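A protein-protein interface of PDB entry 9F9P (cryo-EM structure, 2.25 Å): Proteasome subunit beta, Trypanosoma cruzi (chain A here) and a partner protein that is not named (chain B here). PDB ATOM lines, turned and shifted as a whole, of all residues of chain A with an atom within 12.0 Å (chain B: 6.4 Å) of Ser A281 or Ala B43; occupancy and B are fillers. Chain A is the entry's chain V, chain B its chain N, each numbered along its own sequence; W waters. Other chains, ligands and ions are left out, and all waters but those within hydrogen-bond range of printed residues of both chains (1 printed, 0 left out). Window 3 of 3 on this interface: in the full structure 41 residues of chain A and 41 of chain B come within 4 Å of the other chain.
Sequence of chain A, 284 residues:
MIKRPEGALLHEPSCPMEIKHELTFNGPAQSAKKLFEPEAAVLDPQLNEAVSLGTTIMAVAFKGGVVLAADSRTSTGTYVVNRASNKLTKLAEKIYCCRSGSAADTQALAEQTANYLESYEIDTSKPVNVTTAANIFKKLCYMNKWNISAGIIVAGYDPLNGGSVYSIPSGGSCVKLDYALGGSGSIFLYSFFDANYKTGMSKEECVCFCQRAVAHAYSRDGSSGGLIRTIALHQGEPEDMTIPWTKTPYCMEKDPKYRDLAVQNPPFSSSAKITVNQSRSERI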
ATOM      1  N   ASN A 265      -1.864  26.333  -9.085  1.00  0.00           N
ATOM      2  CA  ASN A 265      -0.459  26.530  -9.441  1.00  0.00           C
ATOM      3  C   ASN A 265      -0.245  27.812 -10.243  1.00  0.00           C
ATOM      4  O   ASN A 265       0.187  27.758 -11.389  1.00  0.00           O
ATOM      5  CB  ASN A 265       0.036  25.370 -10.320  1.00  0.00           C
ATOM      6  CG  ASN A 265      -0.046  24.052  -9.584  1.00  0.00           C
ATOM      7  OD1 ASN A 265       0.289  23.986  -8.393  1.00  0.00           O
ATOM      8  ND2 ASN A 265      -0.534  23.029 -10.253  1.00  0.00           N
ATOM      9  N   PRO A 266      -0.534  28.999  -9.684  1.00  0.00           N
ATOM     10  CA  PRO A 266      -0.378  30.245 -10.439  1.00  0.00           C
ATOM     11  C   PRO A 266       1.093  30.577 -10.668  1.00  0.00           C
ATOM     12  O   PRO A 266       1.916  30.325  -9.794  1.00  0.00           O
ATOM     13  CB  PRO A 266      -1.016  31.311  -9.531  1.00  0.00           C
ATOM     14  CG  PRO A 266      -0.946  30.739  -8.122  1.00  0.00           C
ATOM     15  CD  PRO A 266      -0.926  29.228  -8.279  1.00  0.00           C
ATOM     16  N   PRO A 267       1.449  31.191 -11.807  1.00  0.00           N
ATOM     17  CA  PRO A 267       2.843  31.570 -12.086  1.00  0.00           C
ATOM     18  C   PRO A 267       3.353  32.662 -11.151  1.00  0.00           C
ATOM     19  O   PRO A 267       2.565  33.411 -10.569  1.00  0.00           O
ATOM     20  CB  PRO A 267       2.802  32.101 -13.538  1.00  0.00           C
ATOM     21  CG  PRO A 267       1.375  32.597 -13.707  1.00  0.00           C
ATOM     22  CD  PRO A 267       0.516  31.716 -12.811  1.00  0.00           C
ATOM     23  N   PHE A 268       4.673  32.738 -11.000  1.00  0.00           N
ATOM     24  CA  PHE A 268       5.340  33.770 -10.202  1.00  0.00           C
ATOM     25  C   PHE A 268       5.059  35.161 -10.783  1.00  0.00           C
ATOM     26  O   PHE A 268       5.267  35.365 -11.975  1.00  0.00           O
ATOM     27  CB  PHE A 268       6.838  33.443 -10.180  1.00  0.00           C
ATOM     28  CG  PHE A 268       7.705  34.261  -9.269  1.00  0.00           C
ATOM     29  CD1 PHE A 268       7.317  34.534  -7.963  1.00  0.00           C
ATOM     30  CD2 PHE A 268       8.934  34.729  -9.713  1.00  0.00           C
ATOM     31  CE1 PHE A 268       8.142  35.275  -7.119  1.00  0.00           C
ATOM     32  CE2 PHE A 268       9.769  35.446  -8.860  1.00  0.00           C
ATOM     33  CZ  PHE A 268       9.377  35.712  -7.566  1.00  0.00           C
ATOM     34  N   VAL A 276      -4.749  32.203 -13.824  1.00  0.00           N
ATOM     35  CA  VAL A 276      -4.670  30.929 -14.535  1.00  0.00           C
ATOM     36  C   VAL A 276      -3.551  30.088 -13.919  1.00  0.00           C
ATOM     37  O   VAL A 276      -2.721  30.624 -13.187  1.00  0.00           O
ATOM     38  CB  VAL A 276      -4.408  31.140 -16.045  1.00  0.00           C
ATOM     39  CG1 VAL A 276      -5.534  31.938 -16.697  1.00  0.00           C
ATOM     40  CG2 VAL A 276      -3.039  31.784 -16.333  1.00  0.00           C
ATOM     41  N   ASN A 277      -3.547  28.787 -14.239  1.00  0.00           N
ATOM     42  CA  ASN A 277      -2.462  27.876 -13.891  1.00  0.00           C
ATOM     43  C   ASN A 277      -1.323  28.026 -14.904  1.00  0.00           C
ATOM     44  O   ASN A 277      -1.531  28.190 -16.101  1.00  0.00           O
ATOM     45  CB  ASN A 277      -2.898  26.399 -13.877  1.00  0.00           C
ATOM     46  CG  ASN A 277      -3.699  25.999 -12.658  1.00  0.00           C
ATOM     47  OD1 ASN A 277      -3.197  26.028 -11.536  1.00  0.00           O
ATOM     48  ND2 ASN A 277      -4.955  25.635 -12.863  1.00  0.00           N
ATOM     49  N   GLN A 278      -0.098  27.911 -14.408  1.00  0.00           N
ATOM     50  CA  GLN A 278       1.067  27.876 -15.272  1.00  0.00           C
ATOM     51  C   GLN A 278       1.042  26.606 -16.131  1.00  0.00           C
ATOM     52  O   GLN A 278       0.812  25.507 -15.647  1.00  0.00           O
ATOM     53  CB  GLN A 278       2.316  27.939 -14.389  1.00  0.00           C
ATOM     54  CG  GLN A 278       3.559  28.434 -15.127  1.00  0.00           C
ATOM     55  CD  GLN A 278       4.767  28.384 -14.230  1.00  0.00           C
ATOM     56  OE1 GLN A 278       4.665  28.216 -13.012  1.00  0.00           O
ATOM     57  NE2 GLN A 278       5.928  28.472 -14.851  1.00  0.00           N
ATOM     58  N   SER A 279       1.299  26.736 -17.426  1.00  0.00           N
ATOM     59  CA  SER A 279       1.264  25.569 -18.298  1.00  0.00           C
ATOM     60  C   SER A 279       2.617  25.326 -18.964  1.00  0.00           C
ATOM     61  O   SER A 279       2.836  24.219 -19.437  1.00  0.00           O
ATOM     62  CB  SER A 279       0.133  25.674 -19.355  1.00  0.00           C
ATOM     63  OG  SER A 279       0.312  26.808 -20.207  1.00  0.00           O
ATOM     64  N   ARG A 280       3.486  26.337 -19.058  1.00  0.00           N
ATOM     65  CA  ARG A 280       4.813  26.126 -19.614  1.00  0.00           C
ATOM     66  C   ARG A 280       5.885  26.743 -18.729  1.00  0.00           C
ATOM     67  O   ARG A 280       5.656  27.727 -18.038  1.00  0.00           O
ATOM     68  CB  ARG A 280       4.900  26.628 -21.052  1.00  0.00           C
ATOM     69  CG  ARG A 280       4.215  27.961 -21.295  1.00  0.00           C
ATOM     70  CD  ARG A 280       4.310  28.412 -22.748  1.00  0.00           C
ATOM     71  NE  ARG A 280       4.167  27.297 -23.688  1.00  0.00           N
ATOM     72  CZ  ARG A 280       5.047  26.990 -24.639  1.00  0.00           C
ATOM     73  NH1 ARG A 280       4.848  25.929 -25.404  1.00  0.00           N
ATOM     74  NH2 ARG A 280       6.125  27.738 -24.820  1.00  0.00           N
ATOM     75  N   SER A 281       7.053  26.100 -18.740  1.00  0.00           N
ATOM     76  CA  SER A 281       8.274  26.596 -18.113  1.00  0.00           C
ATOM     77  C   SER A 281       8.502  28.075 -18.438  1.00  0.00           C
ATOM     78  O   SER A 281       8.208  28.503 -19.542  1.00  0.00           O
ATOM     79  CB  SER A 281       9.458  25.760 -18.606  1.00  0.00           C
ATOM     80  OG  SER A 281       9.662  24.597 -17.819  1.00  0.00           O
ATOM     81  N   GLU A 282       9.120  28.834 -17.530  1.00  0.00           N
ATOM     82  CA  GLU A 282       9.541  30.195 -17.858  1.00  0.00           C
ATOM     83  C   GLU A 282      10.799  30.184 -18.750  1.00  0.00           C
ATOM     84  O   GLU A 282      11.860  30.643 -18.282  1.00  0.00           O
ATOM     85  CB  GLU A 282       9.687  31.019 -16.576  1.00  0.00           C
ATOM     86  CG  GLU A 282       8.373  31.674 -16.151  1.00  0.00           C
ATOM     87  CD  GLU A 282       7.916  32.847 -17.015  1.00  0.00           C
ATOM     88  OE1 GLU A 282       7.604  33.920 -16.446  1.00  0.00           O
ATOM     89  OE2 GLU A 282       7.880  32.697 -18.257  1.00  0.00           O
ATOM     90  N   LEU B  40       5.303  22.860 -12.045  1.00  0.00           N
ATOM     91  CA  LEU B  40       6.547  23.310 -12.644  1.00  0.00           C
ATOM     92  C   LEU B  40       7.506  23.876 -11.589  1.00  0.00           C
ATOM     93  O   LEU B  40       7.101  24.578 -10.655  1.00  0.00           O
ATOM     94  CB  LEU B  40       6.224  24.310 -13.742  1.00  0.00           C
ATOM     95  CG  LEU B  40       5.378  23.716 -14.873  1.00  0.00           C
ATOM     96  CD1 LEU B  40       4.984  24.734 -15.925  1.00  0.00           C
ATOM     97  CD2 LEU B  40       6.094  22.609 -15.609  1.00  0.00           C
ATOM     98  N   VAL B  41       8.794  23.570 -11.748  1.00  0.00           N
ATOM     99  CA  VAL B  41       9.800  24.066 -10.826  1.00  0.00           C
ATOM    100  C   VAL B  41      10.933  24.699 -11.628  1.00  0.00           C
ATOM    101  O   VAL B  41      11.688  24.055 -12.333  1.00  0.00           O
ATOM    102  CB  VAL B  41      10.319  22.952  -9.894  1.00  0.00           C
ATOM    103  CG1 VAL B  41      11.379  23.476  -8.946  1.00  0.00           C
ATOM    104  CG2 VAL B  41       9.212  22.311  -9.060  1.00  0.00           C
ATOM    105  N   GLY B  42      11.109  25.992 -11.505  1.00  0.00           N
ATOM    106  CA  GLY B  42      12.160  26.611 -12.283  1.00  0.00           C
ATOM    107  C   GLY B  42      11.930  26.425 -13.779  1.00  0.00           C
ATOM    108  O   GLY B  42      10.795  26.365 -14.260  1.00  0.00           O
ATOM    109  N   ALA B  43      13.026  26.367 -14.520  1.00  0.00           N
ATOM    110  CA  ALA B  43      12.923  26.433 -15.970  1.00  0.00           C
ATOM    111  C   ALA B  43      12.867  25.064 -16.643  1.00  0.00           C
ATOM    112  O   ALA B  43      12.526  24.989 -17.797  1.00  0.00           O
ATOM    113  CB  ALA B  43      14.148  27.180 -16.455  1.00  0.00           C
ATOM    114  N   TYR B  44      13.311  23.996 -15.972  1.00  0.00           N
ATOM    115  CA  TYR B  44      13.561  22.748 -16.664  1.00  0.00           C
ATOM    116  C   TYR B  44      12.837  21.531 -16.082  1.00  0.00           C
ATOM    117  O   TYR B  44      13.063  20.443 -16.593  1.00  0.00           O
ATOM    118  CB  TYR B  44      15.063  22.441 -16.611  1.00  0.00           C
ATOM    119  CG  TYR B  44      15.971  23.534 -17.095  1.00  0.00           C
ATOM    120  CD1 TYR B  44      15.968  23.953 -18.417  1.00  0.00           C
ATOM    121  CD2 TYR B  44      16.827  24.169 -16.208  1.00  0.00           C
ATOM    122  CE1 TYR B  44      16.798  24.991 -18.852  1.00  0.00           C
ATOM    123  CE2 TYR B  44      17.666  25.191 -16.622  1.00  0.00           C
ATOM    124  CZ  TYR B  44      17.630  25.625 -17.935  1.00  0.00           C
ATOM    125  OH  TYR B  44      18.485  26.644 -18.267  1.00  0.00           O
ATOM    126  N   THR B  45      12.002  21.686 -15.041  1.00  0.00           N
ATOM    127  CA  THR B  45      11.659  20.565 -14.171  1.00  0.00           C
ATOM    128  C   THR B  45      10.153  20.522 -13.897  1.00  0.00           C
ATOM    129  O   THR B  45       9.501  21.558 -13.823  1.00  0.00           O
ATOM    130  CB  THR B  45      12.494  20.640 -12.882  1.00  0.00           C
ATOM    131  OG1 THR B  45      13.877  20.774 -13.220  1.00  0.00           O
ATOM    132  CG2 THR B  45      12.388  19.419 -11.987  1.00  0.00           C
ATOM    133  N   VAL B  67      14.335  27.928  -5.693  1.00  0.00           N
ATOM    134  CA  VAL B  67      14.809  28.016  -7.048  1.00  0.00           C
ATOM    135  C   VAL B  67      14.642  29.419  -7.660  1.00  0.00           C
ATOM    136  O   VAL B  67      15.543  29.887  -8.343  1.00  0.00           O
ATOM    137  CB  VAL B  67      14.146  26.897  -7.875  1.00  0.00           C
ATOM    138  CG1 VAL B  67      14.382  27.068  -9.363  1.00  0.00           C
ATOM    139  CG2 VAL B  67      14.642  25.508  -7.438  1.00  0.00           C
ATOM    140  N   ALA B  77      20.441  29.136 -12.654  1.00  0.00           N
ATOM    141  CA  ALA B  77      19.200  28.357 -12.677  1.00  0.00           C
ATOM    142  C   ALA B  77      19.472  26.890 -12.349  1.00  0.00           C
ATOM    143  O   ALA B  77      20.226  26.238 -13.071  1.00  0.00           O
ATOM    144  CB  ALA B  77      18.567  28.480 -14.049  1.00  0.00           C
ATOM    145  N   LEU B  78      18.878  26.353 -11.282  1.00  0.00           N
ATOM    146  CA  LEU B  78      19.143  24.965 -10.922  1.00  0.00           C
ATOM    147  C   LEU B  78      18.625  23.977 -11.975  1.00  0.00           C
ATOM    148  O   LEU B  78      17.511  24.127 -12.482  1.00  0.00           O
ATOM    149  CB  LEU B  78      18.504  24.685  -9.563  1.00  0.00           C
ATOM    150  CG  LEU B  78      19.163  25.434  -8.398  1.00  0.00           C
ATOM    151  CD1 LEU B  78      18.548  25.019  -7.068  1.00  0.00           C
ATOM    152  CD2 LEU B  78      20.651  25.187  -8.376  1.00  0.00           C
ATOM    153  N   CYS B 110      14.426  18.257 -18.474  1.00  0.00           N
ATOM    154  CA  CYS B 110      15.277  18.212 -19.641  1.00  0.00           C
ATOM    155  C   CYS B 110      16.224  19.396 -19.598  1.00  0.00           C
ATOM    156  O   CYS B 110      15.797  20.529 -19.478  1.00  0.00           O
ATOM    157  CB  CYS B 110      14.444  18.257 -20.928  1.00  0.00           C
ATOM    158  SG  CYS B 110      15.369  17.906 -22.455  1.00  0.00           S
ATOM    159  N   ASP B 190      14.703  21.539 -23.569  1.00  0.00           N
ATOM    160  CA  ASP B 190      15.020  22.390 -22.429  1.00  0.00           C
ATOM    161  C   ASP B 190      13.804  23.190 -21.936  1.00  0.00           C
ATOM    162  O   ASP B 190      13.963  24.260 -21.346  1.00  0.00           O
ATOM    163  CB  ASP B 190      16.262  23.236 -22.750  1.00  0.00           C
ATOM    164  CG  ASP B 190      17.586  22.463 -22.717  1.00  0.00           C
ATOM    165  OD1 ASP B 190      17.672  21.367 -23.353  1.00  0.00           O
ATOM    166  OD2 ASP B 190      18.549  22.952 -22.048  1.00  0.00           O
ATOM    167  N   MET B 191      12.591  22.643 -22.092  1.00  0.00           N
ATOM    168  CA  MET B 191      11.406  23.223 -21.481  1.00  0.00           C
ATOM    169  C   MET B 191      10.358  22.139 -21.204  1.00  0.00           C
ATOM    170  O   MET B 191      10.506  21.016 -21.653  1.00  0.00           O
ATOM    171  CB  MET B 191      10.812  24.351 -22.327  1.00  0.00           C
ATOM    172  CG  MET B 191      10.783  24.059 -23.782  1.00  0.00           C
ATOM    173  SD  MET B 191       9.453  24.916 -24.681  1.00  0.00           S
ATOM    174  CE  MET B 191       8.010  24.608 -23.655  1.00  0.00           C
ATOM    175  N   VAL B 192       9.353  22.492 -20.393  1.00  0.00           N
ATOM    176  CA  VAL B 192       8.258  21.626 -20.025  1.00  0.00           C
ATOM    177  C   VAL B 192       6.938  22.263 -20.439  1.00  0.00           C
ATOM    178  O   VAL B 192       6.716  23.413 -20.178  1.00  0.00           O
ATOM    179  CB  VAL B 192       8.281  21.348 -18.509  1.00  0.00           C
ATOM    180  CG1 VAL B 192       7.155  20.403 -18.092  1.00  0.00           C
ATOM    181  CG2 VAL B 192       9.606  20.752 -18.034  1.00  0.00           C
ATOM    182  N   SER B 193       6.043  21.503 -21.055  1.00  0.00           N
ATOM    183  CA  SER B 193       4.661  21.923 -21.236  1.00  0.00           C
ATOM    184  C   SER B 193       3.688  20.902 -20.674  1.00  0.00           C
ATOM    185  O   SER B 193       3.930  19.706 -20.756  1.00  0.00           O
ATOM    186  CB  SER B 193       4.328  22.165 -22.702  1.00  0.00           C
ATOM    187  OG  SER B 193       4.714  21.065 -23.504  1.00  0.00           O
HETATM  188  O   HOH W   1       9.743  23.900 -15.277  1.00  0.00           O
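O of Ala B43 lies within hydrogen-bond range of OG of Ser A281, at 2.9 Å.
O of Val B192 sits at hydrogen-bond distance from N of Ser A281.
NE2 of Gln A278 sits at hydrogen-bond distance from O of Arg A280, 3.3 Å away.
Ser A279 touches Leu B40 (C to CD1, 3.9 Å).
Ser A279 touches Ser B193 (O to CA, 3.4 Å).
C of Arg A280 touches CD1 of Leu B40, 3.6 Å away.
Arg A280 touches Met B191 (NH2 to CE, 3.8 Å).
O of Val B192 touches CA of Arg A280 (3.4 Å).
CD1 of Leu B40 touches N of Ser A281, at 3.8 Å.
Val A276 touches none of the printed residues of chain B.
Of the printed residues of chain B, Ser A279 touches Leu B40 (3.9 Å) and Ser B193 (3.4 Å).
Of the printed residues of chain B, Arg A280 touches Leu B40 (3.6 Å), Met B191 (3.8 Å) and Val B192 (3.4 Å).
Ser A281 touches three residues of chain B.
Printed residues of chain A within 4 Å of Leu B40: Ser A279 (3.9 Å), Arg A280 (3.6 Å) and Ser A281 (3.8 Å).
No residue of chain A comes within 4 Å of Val B41.
No residue of chain A comes within 4 Å of Gly B42.
Of the printed residues of chain A, Ala B43 touches Ser A281.
No residue of chain A comes within 4 Å of Tyr B44.
No residue of chain A comes within 4 Å of Thr B45.
No residue of chain A comes within 4 Å of Ala B77.
Of chain A, only Arg A280 (3.8 Å) comes within 4 Å of Met B191.
Of the printed residues of chain A, Val B192 touches Arg A280 (3.4 Å) and Ser A281 (3.1 Å).
Of chain A, only Ser A279 (3.4 Å) comes within 4 Å of Ser B193.
Among the printed residues, 8 pairs touch across the chains.
Water W1 lies within hydrogen-bond range of the side-chain hydroxyl of Ser A281, the backbone carbonyl oxygen of Thr B45 and the backbone carbonyl oxygen of Gly B42.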
